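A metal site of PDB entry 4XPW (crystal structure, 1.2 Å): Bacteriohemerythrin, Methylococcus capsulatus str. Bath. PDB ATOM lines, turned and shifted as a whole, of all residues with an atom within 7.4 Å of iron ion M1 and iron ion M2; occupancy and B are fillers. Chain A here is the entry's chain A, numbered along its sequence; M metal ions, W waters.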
ATOM      1  N   THR A  13       6.069 -35.482  -3.637  1.00  0.00           N
ATOM      2  CA  THR A  13       7.246 -34.626  -3.570  1.00  0.00           C
ATOM      3  C   THR A  13       8.212 -35.022  -2.476  1.00  0.00           C
ATOM      4  O   THR A  13       9.286 -34.404  -2.396  1.00  0.00           O
ATOM      5  CB  THR A  13       6.848 -33.150  -3.285  1.00  0.00           C
ATOM      6  OG1 THR A  13       6.245 -33.108  -1.959  1.00  0.00           O
ATOM      7  CG2 THR A  13       5.927 -32.568  -4.310  1.00  0.00           C
ATOM      8  N   ALA A  18       3.439 -30.265   1.597  1.00  0.00           N
ATOM      9  CA  ALA A  18       3.150 -29.909   0.222  1.00  0.00           C
ATOM     10  C   ALA A  18       2.230 -30.954  -0.375  1.00  0.00           C
ATOM     11  O   ALA A  18       1.279 -30.638  -1.098  1.00  0.00           O
ATOM     12  CB  ALA A  18       4.452 -29.802  -0.573  1.00  0.00           C
ATOM     13  N   ASP A  19       2.527 -32.226  -0.169  1.00  0.00           N
ATOM     14  CA  ASP A  19       1.632 -33.267  -0.656  1.00  0.00           C
ATOM     15  C   ASP A  19       0.223 -33.085  -0.123  1.00  0.00           C
ATOM     16  O   ASP A  19      -0.752 -33.274  -0.874  1.00  0.00           O
ATOM     17  CB  ASP A  19       2.158 -34.675  -0.225  1.00  0.00           C
ATOM     18  CG  ASP A  19       3.393 -35.072  -1.004  1.00  0.00           C
ATOM     19  OD1 ASP A  19       3.777 -34.571  -2.030  1.00  0.00           O
ATOM     20  OD2 ASP A  19       4.016 -36.051  -0.443  1.00  0.00           O
ATOM     21  N   GLN A  21      -1.233 -30.274   0.912  1.00  0.00           N
ATOM     22  CA  GLN A  21      -1.873 -29.112   0.292  1.00  0.00           C
ATOM     23  C   GLN A  21      -2.248 -29.413  -1.155  1.00  0.00           C
ATOM     24  O   GLN A  21      -3.311 -28.980  -1.625  1.00  0.00           O
ATOM     25  CB  GLN A  21      -0.959 -27.869   0.389  1.00  0.00           C
ATOM     26  CG  GLN A  21      -0.738 -27.418   1.838  1.00  0.00           C
ATOM     27  CD  GLN A  21       0.150 -26.212   1.911  1.00  0.00           C
ATOM     28  OE1 GLN A  21       1.028 -25.977   1.154  1.00  0.00           O
ATOM     29  NE2 GLN A  21      -0.087 -25.388   2.954  1.00  0.00           N
ATOM     30  N   HIS A  22      -1.423 -30.181  -1.873  1.00  0.00           N
ATOM     31  CA  HIS A  22      -1.786 -30.599  -3.228  1.00  0.00           C
ATOM     32  C   HIS A  22      -3.050 -31.428  -3.244  1.00  0.00           C
ATOM     33  O   HIS A  22      -3.923 -31.259  -4.097  1.00  0.00           O
ATOM     34  CB  HIS A  22      -0.624 -31.357  -3.889  1.00  0.00           C
ATOM     35  CG  HIS A  22       0.565 -30.496  -4.121  1.00  0.00           C
ATOM     36  ND1 HIS A  22       1.838 -31.020  -4.232  1.00  0.00           N
ATOM     37  CD2 HIS A  22       0.717 -29.156  -4.267  1.00  0.00           C
ATOM     38  CE1 HIS A  22       2.703 -30.043  -4.471  1.00  0.00           C
ATOM     39  NE2 HIS A  22       2.057 -28.886  -4.479  1.00  0.00           N
ATOM     40  N   ILE A  25      -5.923 -29.090  -2.918  1.00  0.00           N
ATOM     41  CA  ILE A  25      -6.152 -28.420  -4.185  1.00  0.00           C
ATOM     42  C   ILE A  25      -6.922 -29.330  -5.140  1.00  0.00           C
ATOM     43  O   ILE A  25      -7.890 -28.882  -5.787  1.00  0.00           O
ATOM     44  CB  ILE A  25      -4.821 -27.957  -4.795  1.00  0.00           C
ATOM     45  CG1 ILE A  25      -4.281 -26.780  -4.005  1.00  0.00           C
ATOM     46  CG2 ILE A  25      -4.977 -27.548  -6.290  1.00  0.00           C
ATOM     47  CD1 ILE A  25      -2.844 -26.382  -4.286  1.00  0.00           C
ATOM     48  N   HIS A  58      -1.085 -22.019  -0.434  1.00  0.00           N
ATOM     49  CA  HIS A  58      -0.155 -23.118  -0.754  1.00  0.00           C
ATOM     50  C   HIS A  58       1.137 -22.525  -1.324  1.00  0.00           C
ATOM     51  O   HIS A  58       2.230 -22.940  -0.906  1.00  0.00           O
ATOM     52  CB  HIS A  58      -0.821 -24.058  -1.706  1.00  0.00           C
ATOM     53  CG  HIS A  58       0.184 -25.033  -2.339  1.00  0.00           C
ATOM     54  ND1 HIS A  58       0.942 -25.890  -1.570  1.00  0.00           N
ATOM     55  CD2 HIS A  58       0.552 -25.212  -3.636  1.00  0.00           C
ATOM     56  CE1 HIS A  58       1.762 -26.536  -2.409  1.00  0.00           C
ATOM     57  NE2 HIS A  58       1.552 -26.148  -3.669  1.00  0.00           N
ATOM     58  N   PHE A  59       1.030 -21.617  -2.256  1.00  0.00           N
ATOM     59  CA  PHE A  59       2.232 -21.030  -2.845  1.00  0.00           C
ATOM     60  C   PHE A  59       3.035 -20.301  -1.806  1.00  0.00           C
ATOM     61  O   PHE A  59       4.297 -20.413  -1.771  1.00  0.00           O
ATOM     62  CB  PHE A  59       1.851 -20.098  -3.993  1.00  0.00           C
ATOM     63  CG  PHE A  59       1.295 -20.781  -5.212  1.00  0.00           C
ATOM     64  CD1 PHE A  59       0.655 -20.006  -6.173  1.00  0.00           C
ATOM     65  CD2 PHE A  59       1.423 -22.166  -5.427  1.00  0.00           C
ATOM     66  CE1 PHE A  59       0.187 -20.561  -7.338  1.00  0.00           C
ATOM     67  CE2 PHE A  59       0.926 -22.704  -6.625  1.00  0.00           C
ATOM     68  CZ  PHE A  59       0.324 -21.930  -7.568  1.00  0.00           C
ATOM     69  N   GLU A  62       4.965 -22.996   0.272  1.00  0.00           N
ATOM     70  CA  GLU A  62       6.144 -23.487  -0.434  1.00  0.00           C
ATOM     71  C   GLU A  62       7.211 -22.410  -0.529  1.00  0.00           C
ATOM     72  O   GLU A  62       8.427 -22.713  -0.303  1.00  0.00           O
ATOM     73  CB  GLU A  62       5.822 -23.843  -1.893  1.00  0.00           C
ATOM     74  CG  GLU A  62       5.019 -25.144  -2.063  1.00  0.00           C
ATOM     75  CD  GLU A  62       4.920 -25.564  -3.523  1.00  0.00           C
ATOM     76  OE1 GLU A  62       5.364 -24.769  -4.372  1.00  0.00           O
ATOM     77  OE2 GLU A  62       4.386 -26.689  -3.770  1.00  0.00           O
ATOM     78  N   GLU A  63       6.851 -21.192  -0.801  1.00  0.00           N
ATOM     79  CA  GLU A  63       7.846 -20.097  -0.970  1.00  0.00           C
ATOM     80  C   GLU A  63       8.541 -19.822   0.306  1.00  0.00           C
ATOM     81  O   GLU A  63       9.781 -19.598   0.325  1.00  0.00           O
ATOM     82  CB  GLU A  63       7.151 -18.858  -1.511  1.00  0.00           C
ATOM     83  CG  GLU A  63       6.729 -19.018  -2.938  1.00  0.00           C
ATOM     84  CD  GLU A  63       5.762 -18.020  -3.478  1.00  0.00           C
ATOM     85  OE1 GLU A  63       5.711 -16.868  -2.872  1.00  0.00           O
ATOM     86  OE2 GLU A  63       5.079 -18.212  -4.484  1.00  0.00           O
ATOM     87  N   MET A  66      11.063 -22.727   0.791  1.00  0.00           N
ATOM     88  CA  MET A  66      12.162 -22.628  -0.201  1.00  0.00           C
ATOM     89  C   MET A  66      13.064 -21.502   0.160  1.00  0.00           C
ATOM     90  O   MET A  66      14.336 -21.646   0.149  1.00  0.00           O
ATOM     91  CB  MET A  66      11.583 -22.416  -1.622  1.00  0.00           C
ATOM     92  CG  MET A  66      11.014 -23.655  -2.264  1.00  0.00           C
ATOM     93  SD  MET A  66      10.531 -23.431  -3.986  1.00  0.00           S
ATOM     94  CE  MET A  66       9.025 -22.405  -3.846  1.00  0.00           C
ATOM     95  N   HIS A  77      10.928 -20.649  -9.420  1.00  0.00           N
ATOM     96  CA  HIS A  77       9.718 -21.379  -8.968  1.00  0.00           C
ATOM     97  C   HIS A  77       8.681 -20.341  -8.619  1.00  0.00           C
ATOM     98  O   HIS A  77       7.483 -20.447  -9.063  1.00  0.00           O
ATOM     99  CB  HIS A  77      10.130 -22.304  -7.864  1.00  0.00           C
ATOM    100  CG  HIS A  77       9.032 -23.237  -7.443  1.00  0.00           C
ATOM    101  ND1 HIS A  77       9.351 -24.509  -7.034  1.00  0.00           N
ATOM    102  CD2 HIS A  77       7.673 -23.117  -7.319  1.00  0.00           C
ATOM    103  CE1 HIS A  77       8.212 -25.123  -6.699  1.00  0.00           C
ATOM    104  NE2 HIS A  77       7.185 -24.310  -6.833  1.00  0.00           N
ATOM    105  N   LYS A  78       9.026 -19.362  -7.805  1.00  0.00           N
ATOM    106  CA  LYS A  78       8.053 -18.324  -7.454  1.00  0.00           C
ATOM    107  C   LYS A  78       7.553 -17.639  -8.646  1.00  0.00           C
ATOM    108  O   LYS A  78       6.342 -17.235  -8.672  1.00  0.00           O
ATOM    109  CB  LYS A  78       8.705 -17.349  -6.487  1.00  0.00           C
ATOM    110  CG  LYS A  78       7.749 -16.201  -6.120  1.00  0.00           C
ATOM    111  CD  LYS A  78       8.272 -15.392  -4.964  1.00  0.00           C
ATOM    112  CE  LYS A  78       7.373 -14.285  -4.480  1.00  0.00           C
ATOM    113  NZ  LYS A  78       7.126 -13.373  -5.543  1.00  0.00           N
ATOM    114  N   GLU A  80       6.826 -18.865 -11.522  1.00  0.00           N
ATOM    115  CA  GLU A  80       5.717 -19.697 -12.048  1.00  0.00           C
ATOM    116  C   GLU A  80       4.469 -19.526 -11.205  1.00  0.00           C
ATOM    117  O   GLU A  80       3.375 -19.334 -11.774  1.00  0.00           O
ATOM    118  CB  GLU A  80       6.090 -21.196 -12.083  1.00  0.00           C
ATOM    119  CG  GLU A  80       7.386 -21.533 -12.837  1.00  0.00           C
ATOM    120  CD  GLU A  80       7.439 -21.098 -14.254  1.00  0.00           C
ATOM    121  OE1 GLU A  80       6.434 -20.811 -14.900  1.00  0.00           O
ATOM    122  OE2 GLU A  80       8.621 -21.013 -14.806  1.00  0.00           O
ATOM    123  N   HIS A  81       4.607 -19.541  -9.892  1.00  0.00           N
ATOM    124  CA  HIS A  81       3.454 -19.304  -8.995  1.00  0.00           C
ATOM    125  C   HIS A  81       2.832 -17.954  -9.322  1.00  0.00           C
ATOM    126  O   HIS A  81       1.578 -17.813  -9.464  1.00  0.00           O
ATOM    127  CB  HIS A  81       3.888 -19.256  -7.569  1.00  0.00           C
ATOM    128  CG  HIS A  81       4.303 -20.582  -7.007  1.00  0.00           C
ATOM    129  ND1 HIS A  81       4.832 -20.671  -5.747  1.00  0.00           N
ATOM    130  CD2 HIS A  81       4.260 -21.873  -7.464  1.00  0.00           C
ATOM    131  CE1 HIS A  81       5.059 -21.956  -5.463  1.00  0.00           C
ATOM    132  NE2 HIS A  81       4.727 -22.717  -6.499  1.00  0.00           N
ATOM    133  N   TRP A 113      -2.305 -26.999 -15.432  1.00  0.00           N
ATOM    134  CA  TRP A 113      -1.240 -26.271 -14.738  1.00  0.00           C
ATOM    135  C   TRP A 113      -0.649 -27.128 -13.616  1.00  0.00           C
ATOM    136  O   TRP A 113       0.591 -27.251 -13.483  1.00  0.00           O
ATOM    137  CB  TRP A 113      -1.760 -24.905 -14.271  1.00  0.00           C
ATOM    138  CG  TRP A 113      -0.653 -24.024 -13.797  1.00  0.00           C
ATOM    139  CD1 TRP A 113      -0.059 -23.009 -14.570  1.00  0.00           C
ATOM    140  CD2 TRP A 113       0.035 -24.045 -12.564  1.00  0.00           C
ATOM    141  NE1 TRP A 113       0.912 -22.405 -13.827  1.00  0.00           N
ATOM    142  CE2 TRP A 113       1.025 -23.012 -12.601  1.00  0.00           C
ATOM    143  CE3 TRP A 113      -0.134 -24.734 -11.358  1.00  0.00           C
ATOM    144  CZ2 TRP A 113       1.870 -22.732 -11.534  1.00  0.00           C
ATOM    145  CZ3 TRP A 113       0.713 -24.476 -10.275  1.00  0.00           C
ATOM    146  CH2 TRP A 113       1.696 -23.468 -10.381  1.00  0.00           C
ATOM    147  N   PHE A 114      -1.528 -27.679 -12.739  1.00  0.00           N
ATOM    148  CA  PHE A 114      -1.021 -28.420 -11.589  1.00  0.00           C
ATOM    149  C   PHE A 114      -0.366 -29.717 -11.994  1.00  0.00           C
ATOM    150  O   PHE A 114       0.647 -30.115 -11.370  1.00  0.00           O
ATOM    151  CB  PHE A 114      -2.165 -28.726 -10.597  1.00  0.00           C
ATOM    152  CG  PHE A 114      -2.608 -27.490  -9.862  1.00  0.00           C
ATOM    153  CD1 PHE A 114      -1.767 -26.896  -8.979  1.00  0.00           C
ATOM    154  CD2 PHE A 114      -3.857 -26.907 -10.035  1.00  0.00           C
ATOM    155  CE1 PHE A 114      -2.129 -25.650  -8.278  1.00  0.00           C
ATOM    156  CE2 PHE A 114      -4.214 -25.737  -9.307  1.00  0.00           C
ATOM    157  CZ  PHE A 114      -3.292 -25.155  -8.599  1.00  0.00           C
ATOM    158  N   HIS A 117       3.002 -28.614 -13.153  1.00  0.00           N
ATOM    159  CA  HIS A 117       3.833 -27.945 -12.153  1.00  0.00           C
ATOM    160  C   HIS A 117       4.326 -28.904 -11.073  1.00  0.00           C
ATOM    161  O   HIS A 117       5.496 -28.837 -10.643  1.00  0.00           O
ATOM    162  CB  HIS A 117       3.029 -26.830 -11.504  1.00  0.00           C
ATOM    163  CG  HIS A 117       3.805 -26.034 -10.477  1.00  0.00           C
ATOM    164  ND1 HIS A 117       4.634 -24.965 -10.850  1.00  0.00           N
ATOM    165  CD2 HIS A 117       3.869 -26.110  -9.139  1.00  0.00           C
ATOM    166  CE1 HIS A 117       5.152 -24.461  -9.738  1.00  0.00           C
ATOM    167  NE2 HIS A 117       4.720 -25.092  -8.665  1.00  0.00           N
ATOM    168  N   ILE A 118       3.458 -29.782 -10.563  1.00  0.00           N
ATOM    169  CA  ILE A 118       3.863 -30.559  -9.399  1.00  0.00           C
ATOM    170  C   ILE A 118       5.034 -31.515  -9.777  1.00  0.00           C
ATOM    171  O   ILE A 118       6.003 -31.544  -9.084  1.00  0.00           O
ATOM    172  CB  ILE A 118       2.641 -31.254  -8.775  1.00  0.00           C
ATOM    173  CG1 ILE A 118       1.738 -30.178  -8.153  1.00  0.00           C
ATOM    174  CG2 ILE A 118       3.123 -32.248  -7.693  1.00  0.00           C
ATOM    175  CD1 ILE A 118       0.324 -30.713  -7.761  1.00  0.00           C
ATOM    176  N   VAL A 121       8.206 -29.107 -11.367  1.00  0.00           N
ATOM    177  CA  VAL A 121       8.667 -27.963 -10.609  1.00  0.00           C
ATOM    178  C   VAL A 121       8.722 -28.307  -9.131  1.00  0.00           C
ATOM    179  O   VAL A 121       9.787 -28.223  -8.479  1.00  0.00           O
ATOM    180  CB  VAL A 121       7.869 -26.654 -10.917  1.00  0.00           C
ATOM    181  CG1 VAL A 121       8.516 -25.477 -10.251  1.00  0.00           C
ATOM    182  CG2 VAL A 121       7.744 -26.435 -12.435  1.00  0.00           C
ATOM    183  N   ASP A 122       7.572 -28.736  -8.552  1.00  0.00           N
ATOM    184  CA  ASP A 122       7.562 -29.011  -7.113  1.00  0.00           C
ATOM    185  C   ASP A 122       8.433 -30.187  -6.743  1.00  0.00           C
ATOM    186  O   ASP A 122       9.131 -30.162  -5.727  1.00  0.00           O
ATOM    187  CB  ASP A 122       6.143 -29.228  -6.572  1.00  0.00           C
ATOM    188  CG  ASP A 122       5.312 -27.983  -6.514  1.00  0.00           C
ATOM    189  OD1 ASP A 122       5.872 -26.858  -6.574  1.00  0.00           O
ATOM    190  OD2 ASP A 122       4.073 -28.155  -6.304  1.00  0.00           O
ATOM    191  N   LYS A 123       8.423 -31.271  -7.524  1.00  0.00           N
ATOM    192  CA  LYS A 123       9.264 -32.415  -7.080  1.00  0.00           C
ATOM    193  C   LYS A 123      10.702 -32.025  -6.936  1.00  0.00           C
ATOM    194  O   LYS A 123      11.436 -32.661  -6.125  1.00  0.00           O
ATOM    195  CB  LYS A 123       9.155 -33.567  -8.062  1.00  0.00           C
ATOM    196  CG  LYS A 123       7.891 -34.374  -7.937  1.00  0.00           C
ATOM    197  CD  LYS A 123       7.869 -35.598  -8.886  1.00  0.00           C
ATOM    198  CE  LYS A 123       6.621 -36.382  -8.805  1.00  0.00           C
ATOM    199  NZ  LYS A 123       6.764 -37.655  -9.544  1.00  0.00           N
ATOM    200  N   TYR A 125      12.064 -29.614  -5.393  1.00  0.00           N
ATOM    201  CA  TYR A 125      12.461 -29.169  -4.077  1.00  0.00           C
ATOM    202  C   TYR A 125      12.513 -30.240  -3.034  1.00  0.00           C
ATOM    203  O   TYR A 125      12.823 -29.989  -1.901  1.00  0.00           O
ATOM    204  CB  TYR A 125      11.586 -27.988  -3.605  1.00  0.00           C
ATOM    205  CG  TYR A 125      10.100 -28.175  -3.424  1.00  0.00           C
ATOM    206  CD1 TYR A 125       9.571 -29.313  -2.758  1.00  0.00           C
ATOM    207  CD2 TYR A 125       9.230 -27.234  -3.937  1.00  0.00           C
ATOM    208  CE1 TYR A 125       8.178 -29.471  -2.637  1.00  0.00           C
ATOM    209  CE2 TYR A 125       7.847 -27.400  -3.806  1.00  0.00           C
ATOM    210  CZ  TYR A 125       7.351 -28.516  -3.211  1.00  0.00           C
ATOM    211  OH  TYR A 125       5.967 -28.784  -3.122  1.00  0.00           O
HETATM  212 FE    FE M   1       2.725 -26.946  -5.283  1.00  0.00          FE
HETATM  213 FE    FE M   2       5.058 -24.871  -6.524  1.00  0.00          FE
HETATM  214  O   HOH W   1       0.863 -26.967  -6.837  1.00  0.00           O
HETATM  215  O   HOH W   2       3.238 -25.266  -6.057  1.00  0.00           O
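Iron ion M2 is bound by water W2, 1.9 Å away. OD1 of Asp 122 binds iron ion M2, at 2.1 Å. Iron ion M2 is bound by OE1 of Glu 62, 2.2 Å away. NE2 of His 117 is bound to iron ion M2 (2.2 Å). Iron ion M2 is bound by a ring nitrogen (NE2) of His 81, 2.2 Å away. NE2 of His 77 binds iron ion M2 (2.2 Å). Iron ion M2 has six donor atoms within binding distance.
OE2 of Glu 62 lies close to OH of Tyr 125 (2.7 Å). ND1 of His 22 sits close to O of Ala 18 (3.2 Å). OE1 of Gln 21 lies within hydrogen-bond range of ND1 of His 58 (2.7 Å). ND1 of His 81 lies within hydrogen-bond range of OE2 of Glu 63 (2.8 Å). A ring nitrogen (ND1) of His 77 sits at hydrogen-bond distance from the side-chain sulfur of Met 66 (3.4 Å).
Iron ion M1 is bound by water W2, at 1.9 Å. The side-chain carboxylate (OD2) of Asp 122 binds iron ion M1, at 2.1 Å. A ring nitrogen (NE2) of His 58 is bound to iron ion M1 (2.1 Å). NE2 of His 22 binds iron ion M1 (2.2 Å). Iron ion M1 is bound by the side-chain carboxylate (OE2) of Glu 62. Iron ion M1 is bound by water W1 (2.4 Å).
Five residues have an atom within 4 Å of iron ion M2: Glu 62, His 77, His 81, His 117 and Asp 122. Along chain A the residues within 4 Å of iron ion M2 span positions 62 to 122.
Within 4 Å of iron ion M1: His 22, His 58, Glu 62 and Asp 122. The nearest printed residue that does not touch iron ion M1 is His 117 (4.1 Å).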
